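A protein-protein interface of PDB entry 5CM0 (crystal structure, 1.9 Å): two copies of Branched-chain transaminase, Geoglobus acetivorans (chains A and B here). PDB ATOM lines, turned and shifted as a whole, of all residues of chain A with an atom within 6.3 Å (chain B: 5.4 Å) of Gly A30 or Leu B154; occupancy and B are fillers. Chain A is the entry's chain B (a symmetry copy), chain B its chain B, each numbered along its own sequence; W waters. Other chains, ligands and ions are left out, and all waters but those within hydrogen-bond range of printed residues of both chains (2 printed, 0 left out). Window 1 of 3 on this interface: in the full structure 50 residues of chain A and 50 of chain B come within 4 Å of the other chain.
Water W2 lies within hydrogen-bond range of O of Asn A155 (2.9 Å), ND2 of Asn B155 (2.9 Å) and N of Leu A157 (3.3 Å).
Water W1 lies within hydrogen-bond range of the backbone carbonyl oxygen (O) of Asn B155 (2.9 Å), the side-chain amide nitrogen (ND2) of Asn A155 (2.9 Å) and the backbone NH (N) of Leu B157 (3.3 Å).
Of chain B, only Leu B154 (3.1 Å) comes within 4 Å of Gly A30.
Leu B154 touches just these residues of chain A: Phe A27 (3.6 Å), Leu A28 (3.2 Å), Tyr A29 (2.8 Å) and Gly A30 (3.1 Å).
Of the printed residues of chain B, Leu A157 touches Asp B31 (3.6 Å), Ser B153 (3.6 Å) and Asn B155 (3.0 Å).
Printed residues of chain A within 4 Å of Gly B26: Phe A27.
Of the printed residues of chain B, Asp A31 touches Leu B157.
Of the printed residues of chain A, Asp B31 touches Leu A157.
The nearest residue of chain B that does not touch Gly A30 is Leu B157 (4.2 Å).
The nearest residue of chain A that does not touch Leu B154 is Asn A155 (4.3 Å).
Along chain B the printed residues that touch a printed residue of chain A span positions 26 to 157.
Printed residues of chain A that touch a printed residue of chain B: Phe A27, Leu A28, Tyr A29, Gly A30, Asp A31, Ile A61, Ser A153, Leu A154, Asn A155 and Leu A157.
Hydrophobic or aromatic side chains of chain A within 4 Å of the printed part of chain B: Phe A27, Leu A28, Tyr A29, Ile A61 and Leu A157.
Among the printed residues, 20 pairs touch across the chains.
The backbone NH of Tyr B156 is in hydrogen-bond range of the backbone carbonyl oxygen of Tyr A29.
The backbone NH of Leu B157 lies close to the side-chain amide nitrogen of Asn A155 (3.0 Å).
The backbone carbonyl oxygen (O) of Tyr A29 sits close to the backbone carbonyl oxygen (O) of Leu B154 (3.0 Å).
The backbone carbonyl oxygen (O) of Leu B154 is in hydrogen-bond range of the backbone NH (N) of Gly A30 (3.1 Å).
The side-chain amide nitrogen (ND2) of Asn A155 sits close to the backbone NH (N) of Tyr B156 (3.2 Å).
The backbone NH of Gly B30 is in hydrogen-bond range of the backbone carbonyl oxygen of Leu A154.
The side-chain amide nitrogen (ND2) of Asn B155 sits close to the backbone NH (N) of Leu A157, 3.0 Å away.
The backbone carbonyl oxygen (O) of His A25 lies within hydrogen-bond range of the backbone NH (N) of Gly A30 (3.4 Å).
N of Asn B155 lies within hydrogen-bond range of OG of Ser B153 (2.8 Å).
OD1 of Asn A155 lies close to O of Gly A30 (2.9 Å).
The backbone carbonyl oxygen (O) of Tyr A29 lies close to the side-chain amide oxygen (OD1) of Asn A155.
The backbone NH (N) of Leu B154 is in hydrogen-bond range of the backbone carbonyl oxygen (O) of Gly B32 (2.9 Å).
O of Gly A32 lies within hydrogen-bond range of N of Leu A154.
Among the printed residues, merely in contact across the chains: Phe A27 with Gly B26, Phe A27 with Ile B93, Phe A27 with Thr B95, Phe A27 with Leu B154, Leu A28 with Ile B93, Leu A28 with Leu B154, Tyr A29 with Leu B157, Asp A31 with Leu B157, Ile A61 with Leu B157, Ser A153 with Leu B157, Asn A155 with Asn B155, Leu A157 with Asp B31 and Leu A157 with Ser B153.
Gly A30 touches Leu B154, and with the chains exchanged Leu A154 touches Gly B30.
Asp A31 touches Leu B157, and with the chains exchanged Leu A157 touches Asp B31.
Ser A153 touches Leu B157, and with the chains exchanged Leu A157 touches Ser B153.
Asn A155 touches Leu B157, and with the chains exchanged Leu A157 touches Asn B155.
Of the 20 pairs that touch across the chains among the printed residues, 9 have their exchanged pair printed and touching as well.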
ATOM      1  N   HIS A  25      30.588 -17.203 -21.801  1.00  0.00           N
ATOM      2  CA  HIS A  25      30.431 -15.944 -22.542  1.00  0.00           C
ATOM      3  C   HIS A  25      29.126 -15.205 -22.239  1.00  0.00           C
ATOM      4  O   HIS A  25      29.032 -14.001 -22.552  1.00  0.00           O
ATOM      5  CB  HIS A  25      30.593 -16.193 -24.020  1.00  0.00           C
ATOM      6  CG  HIS A  25      32.008 -16.383 -24.443  1.00  0.00           C
ATOM      7  ND1 HIS A  25      32.436 -16.158 -25.732  1.00  0.00           N
ATOM      8  CD2 HIS A  25      33.099 -16.783 -23.746  1.00  0.00           C
ATOM      9  CE1 HIS A  25      33.730 -16.397 -25.814  1.00  0.00           C
ATOM     10  NE2 HIS A  25      34.160 -16.759 -24.616  1.00  0.00           N
ATOM     11  N   GLY A  26      28.129 -15.905 -21.667  1.00  0.00           N
ATOM     12  CA  GLY A  26      26.919 -15.311 -21.123  1.00  0.00           C
ATOM     13  C   GLY A  26      27.235 -14.258 -20.067  1.00  0.00           C
ATOM     14  O   GLY A  26      26.657 -13.170 -20.051  1.00  0.00           O
ATOM     15  N   PHE A  27      28.200 -14.588 -19.211  1.00  0.00           N
ATOM     16  CA  PHE A  27      28.717 -13.709 -18.183  1.00  0.00           C
ATOM     17  C   PHE A  27      29.711 -12.679 -18.704  1.00  0.00           C
ATOM     18  O   PHE A  27      29.578 -11.494 -18.382  1.00  0.00           O
ATOM     19  CB  PHE A  27      29.355 -14.524 -17.071  1.00  0.00           C
ATOM     20  CG  PHE A  27      29.893 -13.702 -15.938  1.00  0.00           C
ATOM     21  CD1 PHE A  27      29.022 -13.028 -15.094  1.00  0.00           C
ATOM     22  CD2 PHE A  27      31.251 -13.621 -15.701  1.00  0.00           C
ATOM     23  CE1 PHE A  27      29.502 -12.318 -14.023  1.00  0.00           C
ATOM     24  CE2 PHE A  27      31.738 -12.877 -14.641  1.00  0.00           C
ATOM     25  CZ  PHE A  27      30.866 -12.225 -13.814  1.00  0.00           C
ATOM     26  N   LEU A  28      30.691 -13.094 -19.519  1.00  0.00           N
ATOM     27  CA  LEU A  28      31.717 -12.180 -19.948  1.00  0.00           C
ATOM     28  C   LEU A  28      31.232 -11.067 -20.921  1.00  0.00           C
ATOM     29  O   LEU A  28      31.757  -9.944 -20.906  1.00  0.00           O
ATOM     30  CB  LEU A  28      32.830 -12.954 -20.656  1.00  0.00           C
ATOM     31  CG  LEU A  28      33.717 -13.881 -19.808  1.00  0.00           C
ATOM     32  CD1 LEU A  28      34.760 -14.566 -20.679  1.00  0.00           C
ATOM     33  CD2 LEU A  28      34.407 -13.090 -18.715  1.00  0.00           C
ATOM     34  N   TYR A  29      30.274 -11.452 -21.750  1.00  0.00           N
ATOM     35  CA  TYR A  29      29.819 -10.678 -22.900  1.00  0.00           C
ATOM     36  C   TYR A  29      28.330 -10.531 -23.036  1.00  0.00           C
ATOM     37  O   TYR A  29      27.873  -9.936 -24.030  1.00  0.00           O
ATOM     38  CB  TYR A  29      30.364 -11.308 -24.171  1.00  0.00           C
ATOM     39  CG  TYR A  29      31.874 -11.397 -24.168  1.00  0.00           C
ATOM     40  CD1 TYR A  29      32.651 -10.296 -23.900  1.00  0.00           C
ATOM     41  CD2 TYR A  29      32.521 -12.626 -24.366  1.00  0.00           C
ATOM     42  CE1 TYR A  29      34.030 -10.377 -23.888  1.00  0.00           C
ATOM     43  CE2 TYR A  29      33.921 -12.724 -24.363  1.00  0.00           C
ATOM     44  CZ  TYR A  29      34.662 -11.612 -24.147  1.00  0.00           C
ATOM     45  OH  TYR A  29      36.016 -11.653 -24.054  1.00  0.00           O
ATOM     46  N   GLY A  30      27.545 -11.016 -22.055  1.00  0.00           N
ATOM     47  CA  GLY A  30      26.089 -10.975 -22.202  1.00  0.00           C
ATOM     48  C   GLY A  30      25.649 -11.796 -23.415  1.00  0.00           C
ATOM     49  O   GLY A  30      24.624 -11.508 -24.036  1.00  0.00           O
ATOM     50  N   ASP A  31      26.447 -12.836 -23.745  1.00  0.00           N
ATOM     51  CA  ASP A  31      26.243 -13.498 -25.024  1.00  0.00           C
ATOM     52  C   ASP A  31      25.255 -14.675 -24.881  1.00  0.00           C
ATOM     53  O   ASP A  31      25.644 -15.824 -24.673  1.00  0.00           O
ATOM     54  CB  ASP A  31      27.576 -13.993 -25.591  1.00  0.00           C
ATOM     55  CG  ASP A  31      27.430 -14.605 -26.970  1.00  0.00           C
ATOM     56  OD1 ASP A  31      26.298 -14.630 -27.495  1.00  0.00           O
ATOM     57  OD2 ASP A  31      28.392 -15.089 -27.605  1.00  0.00           O
ATOM     58  N   GLY A  32      23.920 -14.388 -24.917  1.00  0.00           N
ATOM     59  CA  GLY A  32      22.806 -15.338 -24.699  1.00  0.00           C
ATOM     60  C   GLY A  32      21.476 -14.640 -24.785  1.00  0.00           C
ATOM     61  O   GLY A  32      21.405 -13.392 -25.045  1.00  0.00           O
ATOM     62  N   VAL A  33      20.438 -15.435 -24.655  1.00  0.00           N
ATOM     63  CA  VAL A  33      19.051 -15.031 -24.800  1.00  0.00           C
ATOM     64  C   VAL A  33      18.225 -15.530 -23.586  1.00  0.00           C
ATOM     65  O   VAL A  33      18.647 -16.443 -22.860  1.00  0.00           O
ATOM     66  CB  VAL A  33      18.380 -15.499 -26.114  1.00  0.00           C
ATOM     67  CG1 VAL A  33      19.026 -14.804 -27.316  1.00  0.00           C
ATOM     68  CG2 VAL A  33      18.445 -17.028 -26.301  1.00  0.00           C
ATOM     69  N   ILE A  61      21.127 -14.555 -32.918  1.00  0.00           N
ATOM     70  CA  ILE A  61      22.472 -14.457 -32.453  1.00  0.00           C
ATOM     71  C   ILE A  61      23.308 -15.688 -32.859  1.00  0.00           C
ATOM     72  O   ILE A  61      24.424 -15.847 -32.380  1.00  0.00           O
ATOM     73  CB  ILE A  61      22.610 -14.118 -30.971  1.00  0.00           C
ATOM     74  CG1 ILE A  61      22.139 -15.224 -30.032  1.00  0.00           C
ATOM     75  CG2 ILE A  61      21.932 -12.778 -30.695  1.00  0.00           C
ATOM     76  CD1 ILE A  61      22.557 -15.015 -28.568  1.00  0.00           C
ATOM     77  N   SER A 153      17.865 -10.433 -25.284  1.00  0.00           N
ATOM     78  CA  SER A 153      19.212 -10.937 -25.067  1.00  0.00           C
ATOM     79  C   SER A 153      19.641 -10.637 -23.651  1.00  0.00           C
ATOM     80  O   SER A 153      19.011  -9.823 -23.006  1.00  0.00           O
ATOM     81  CB  SER A 153      20.167 -10.302 -26.071  1.00  0.00           C
ATOM     82  OG  SER A 153      20.737  -9.102 -25.575  1.00  0.00           O
ATOM     83  N   LEU A 154      20.794 -11.148 -23.248  1.00  0.00           N
ATOM     84  CA  LEU A 154      21.393 -10.806 -21.959  1.00  0.00           C
ATOM     85  C   LEU A 154      22.078  -9.435 -21.979  1.00  0.00           C
ATOM     86  O   LEU A 154      22.672  -9.035 -20.982  1.00  0.00           O
ATOM     87  CB  LEU A 154      22.418 -11.894 -21.520  1.00  0.00           C
ATOM     88  CG  LEU A 154      21.823 -13.330 -21.328  1.00  0.00           C
ATOM     89  CD1 LEU A 154      22.946 -14.285 -20.867  1.00  0.00           C
ATOM     90  CD2 LEU A 154      20.649 -13.370 -20.353  1.00  0.00           C
ATOM     91  N   ASN A 155      22.075  -8.739 -23.121  1.00  0.00           N
ATOM     92  CA  ASN A 155      22.636  -7.385 -23.191  1.00  0.00           C
ATOM     93  C   ASN A 155      21.491  -6.417 -22.805  1.00  0.00           C
ATOM     94  O   ASN A 155      20.759  -5.944 -23.686  1.00  0.00           O
ATOM     95  CB  ASN A 155      23.196  -7.043 -24.596  1.00  0.00           C
ATOM     96  CG  ASN A 155      24.606  -7.545 -24.809  1.00  0.00           C
ATOM     97  OD1 ASN A 155      24.971  -8.671 -24.410  1.00  0.00           O
ATOM     98  ND2 ASN A 155      25.370  -6.774 -25.434  1.00  0.00           N
ATOM     99  N   LEU A 157      21.877  -3.557 -20.673  1.00  0.00           N
ATOM    100  CA  LEU A 157      22.374  -2.317 -20.156  1.00  0.00           C
ATOM    101  C   LEU A 157      21.734  -1.064 -20.743  1.00  0.00           C
ATOM    102  O   LEU A 157      21.537  -0.084 -20.013  1.00  0.00           O
ATOM    103  CB  LEU A 157      23.889  -2.267 -20.231  1.00  0.00           C
ATOM    104  CG  LEU A 157      24.721  -1.359 -19.331  1.00  0.00           C
ATOM    105  CD1 LEU A 157      24.369  -1.455 -17.830  1.00  0.00           C
ATOM    106  CD2 LEU A 157      26.194  -1.724 -19.536  1.00  0.00           C
ATOM    107  N   GLY B  26      25.182  -9.239 -13.555  1.00  0.00           N
ATOM    108  CA  GLY B  26      26.259  -9.377 -14.523  1.00  0.00           C
ATOM    109  C   GLY B  26      25.948 -10.451 -15.560  1.00  0.00           C
ATOM    110  O   GLY B  26      26.152 -10.263 -16.760  1.00  0.00           O
ATOM    111  N   GLY B  30      24.132  -8.564 -18.334  1.00  0.00           N
ATOM    112  CA  GLY B  30      25.405  -7.983 -18.763  1.00  0.00           C
ATOM    113  C   GLY B  30      25.715  -6.716 -17.964  1.00  0.00           C
ATOM    114  O   GLY B  30      26.388  -5.808 -18.454  1.00  0.00           O
ATOM    115  N   ASP B  31      25.208  -6.670 -16.712  1.00  0.00           N
ATOM    116  CA  ASP B  31      25.236  -5.407 -15.990  1.00  0.00           C
ATOM    117  C   ASP B  31      26.531  -5.277 -15.163  1.00  0.00           C
ATOM    118  O   ASP B  31      26.582  -5.623 -13.982  1.00  0.00           O
ATOM    119  CB  ASP B  31      24.012  -5.282 -15.080  1.00  0.00           C
ATOM    120  CG  ASP B  31      23.943  -3.940 -14.379  1.00  0.00           C
ATOM    121  OD1 ASP B  31      24.836  -3.099 -14.612  1.00  0.00           O
ATOM    122  OD2 ASP B  31      23.034  -3.638 -13.576  1.00  0.00           O
ATOM    123  N   GLY B  32      27.651  -4.832 -15.805  1.00  0.00           N
ATOM    124  CA  GLY B  32      29.014  -4.729 -15.236  1.00  0.00           C
ATOM    125  C   GLY B  32      29.991  -4.228 -16.264  1.00  0.00           C
ATOM    126  O   GLY B  32      29.607  -3.926 -17.444  1.00  0.00           O
ATOM    127  N   VAL B  33      31.214  -4.061 -15.812  1.00  0.00           N
ATOM    128  CA  VAL B  33      32.315  -3.493 -16.569  1.00  0.00           C
ATOM    129  C   VAL B  33      33.559  -4.414 -16.464  1.00  0.00           C
ATOM    130  O   VAL B  33      33.653  -5.258 -15.560  1.00  0.00           O
ATOM    131  CB  VAL B  33      32.701  -2.051 -16.159  1.00  0.00           C
ATOM    132  CG1 VAL B  33      31.566  -1.081 -16.503  1.00  0.00           C
ATOM    133  CG2 VAL B  33      33.050  -1.933 -14.662  1.00  0.00           C
ATOM    134  N   PHE B  34      34.439  -4.289 -17.449  1.00  0.00           N
ATOM    135  CA  PHE B  34      35.684  -5.056 -17.492  1.00  0.00           C
ATOM    136  C   PHE B  34      36.839  -4.322 -18.058  1.00  0.00           C
ATOM    137  O   PHE B  34      36.710  -3.233 -18.733  1.00  0.00           O
ATOM    138  CB  PHE B  34      35.468  -6.394 -18.208  1.00  0.00           C
ATOM    139  CG  PHE B  34      35.469  -6.331 -19.704  1.00  0.00           C
ATOM    140  CD1 PHE B  34      34.282  -6.032 -20.390  1.00  0.00           C
ATOM    141  CD2 PHE B  34      36.639  -6.588 -20.448  1.00  0.00           C
ATOM    142  CE1 PHE B  34      34.224  -6.038 -21.770  1.00  0.00           C
ATOM    143  CE2 PHE B  34      36.589  -6.559 -21.835  1.00  0.00           C
ATOM    144  CZ  PHE B  34      35.376  -6.256 -22.503  1.00  0.00           C
ATOM    145  N   ILE B  93      36.771  -7.798 -13.745  1.00  0.00           N
ATOM    146  CA  ILE B  93      35.371  -7.637 -13.975  1.00  0.00           C
ATOM    147  C   ILE B  93      34.740  -7.094 -12.670  1.00  0.00           C
ATOM    148  O   ILE B  93      35.048  -7.619 -11.580  1.00  0.00           O
ATOM    149  CB  ILE B  93      34.723  -8.985 -14.281  1.00  0.00           C
ATOM    150  CG1 ILE B  93      35.334  -9.597 -15.553  1.00  0.00           C
ATOM    151  CG2 ILE B  93      33.231  -8.880 -14.427  1.00  0.00           C
ATOM    152  CD1 ILE B  93      34.921 -10.998 -15.841  1.00  0.00           C
ATOM    153  N   VAL B  94      33.859  -6.073 -12.754  1.00  0.00           N
ATOM    154  CA  VAL B  94      32.983  -5.709 -11.613  1.00  0.00           C
ATOM    155  C   VAL B  94      31.573  -5.754 -12.072  1.00  0.00           C
ATOM    156  O   VAL B  94      31.241  -5.132 -13.083  1.00  0.00           O
ATOM    157  CB  VAL B  94      33.311  -4.347 -10.987  1.00  0.00           C
ATOM    158  CG1 VAL B  94      32.478  -4.108  -9.702  1.00  0.00           C
ATOM    159  CG2 VAL B  94      34.805  -4.175 -10.712  1.00  0.00           C
ATOM    160  N   THR B  95      30.755  -6.534 -11.377  1.00  0.00           N
ATOM    161  CA  THR B  95      29.358  -6.613 -11.649  1.00  0.00           C
ATOM    162  C   THR B  95      28.506  -5.954 -10.571  1.00  0.00           C
ATOM    163  O   THR B  95      28.931  -5.783  -9.410  1.00  0.00           O
ATOM    164  CB  THR B  95      28.840  -8.051 -11.872  1.00  0.00           C
ATOM    165  OG1 THR B  95      28.628  -8.741 -10.618  1.00  0.00           O
ATOM    166  CG2 THR B  95      29.814  -8.785 -12.759  1.00  0.00           C
ATOM    167  N   LYS B 152      33.454   0.046 -21.510  1.00  0.00           N
ATOM    168  CA  LYS B 152      33.928  -1.337 -21.640  1.00  0.00           C
ATOM    169  C   LYS B 152      33.075  -2.235 -20.758  1.00  0.00           C
ATOM    170  O   LYS B 152      33.468  -2.582 -19.599  1.00  0.00           O
ATOM    171  CB  LYS B 152      35.431  -1.362 -21.270  1.00  0.00           C
ATOM    172  CG  LYS B 152      36.115  -2.523 -21.995  1.00  0.00           C
ATOM    173  CD  LYS B 152      37.616  -2.286 -22.015  1.00  0.00           C
ATOM    174  CE  LYS B 152      38.448  -3.432 -22.631  1.00  0.00           C
ATOM    175  NZ  LYS B 152      38.291  -3.382 -24.066  1.00  0.00           N
ATOM    176  N   SER B 153      31.875  -2.552 -21.227  1.00  0.00           N
ATOM    177  CA  SER B 153      30.860  -3.178 -20.395  1.00  0.00           C
ATOM    178  C   SER B 153      30.775  -4.649 -20.724  1.00  0.00           C
ATOM    179  O   SER B 153      31.284  -5.053 -21.750  1.00  0.00           O
ATOM    180  CB  SER B 153      29.516  -2.492 -20.617  1.00  0.00           C
ATOM    181  OG  SER B 153      28.774  -3.105 -21.659  1.00  0.00           O
ATOM    182  N   LEU B 154      29.991  -5.394 -19.960  1.00  0.00           N
ATOM    183  CA  LEU B 154      29.702  -6.795 -20.267  1.00  0.00           C
ATOM    184  C   LEU B 154      28.659  -6.946 -21.380  1.00  0.00           C
ATOM    185  O   LEU B 154      28.277  -8.065 -21.709  1.00  0.00           O
ATOM    186  CB  LEU B 154      29.219  -7.550 -18.994  1.00  0.00           C
ATOM    187  CG  LEU B 154      30.248  -7.593 -17.814  1.00  0.00           C
ATOM    188  CD1 LEU B 154      29.642  -8.396 -16.643  1.00  0.00           C
ATOM    189  CD2 LEU B 154      31.603  -8.169 -18.217  1.00  0.00           C
ATOM    190  N   ASN B 155      28.132  -5.838 -21.913  1.00  0.00           N
ATOM    191  CA  ASN B 155      27.194  -5.905 -23.038  1.00  0.00           C
ATOM    192  C   ASN B 155      28.053  -5.901 -24.325  1.00  0.00           C
ATOM    193  O   ASN B 155      28.331  -4.829 -24.880  1.00  0.00           O
ATOM    194  CB  ASN B 155      26.187  -4.725 -23.045  1.00  0.00           C
ATOM    195  CG  ASN B 155      24.993  -4.960 -22.148  1.00  0.00           C
ATOM    196  OD1 ASN B 155      25.112  -5.481 -21.018  1.00  0.00           O
ATOM    197  ND2 ASN B 155      23.889  -4.574 -22.597  1.00  0.00           N
ATOM    198  N   TYR B 156      28.502  -7.071 -24.767  1.00  0.00           N
ATOM    199  CA  TYR B 156      29.388  -7.122 -25.978  1.00  0.00           C
ATOM    200  C   TYR B 156      28.768  -7.851 -27.169  1.00  0.00           C
ATOM    201  O   TYR B 156      29.487  -8.236 -28.109  1.00  0.00           O
ATOM    202  CB  TYR B 156      30.807  -7.668 -25.576  1.00  0.00           C
ATOM    203  CG  TYR B 156      31.809  -6.544 -25.518  1.00  0.00           C
ATOM    204  CD1 TYR B 156      31.532  -5.437 -24.728  1.00  0.00           C
ATOM    205  CD2 TYR B 156      32.982  -6.565 -26.205  1.00  0.00           C
ATOM    206  CE1 TYR B 156      32.364  -4.367 -24.649  1.00  0.00           C
ATOM    207  CE2 TYR B 156      33.860  -5.517 -26.108  1.00  0.00           C
ATOM    208  CZ  TYR B 156      33.526  -4.399 -25.337  1.00  0.00           C
ATOM    209  OH  TYR B 156      34.279  -3.209 -25.221  1.00  0.00           O
ATOM    210  N   LEU B 157      27.435  -7.973 -27.189  1.00  0.00           N
ATOM    211  CA  LEU B 157      26.754  -8.583 -28.291  1.00  0.00           C
ATOM    212  C   LEU B 157      26.795  -7.798 -29.596  1.00  0.00           C
ATOM    213  O   LEU B 157      26.883  -8.408 -30.670  1.00  0.00           O
ATOM    214  CB  LEU B 157      25.337  -8.967 -27.906  1.00  0.00           C
ATOM    215  CG  LEU B 157      24.557 -10.052 -28.642  1.00  0.00           C
ATOM    216  CD1 LEU B 157      25.327 -11.379 -28.822  1.00  0.00           C
ATOM    217  CD2 LEU B 157      23.267 -10.310 -27.858  1.00  0.00           C
HETATM  218  O   HOH W   1      26.572  -4.738 -27.163  1.00  0.00           O
HETATM  219  O   HOH W   2      21.696  -3.235 -24.002  1.00  0.00           O
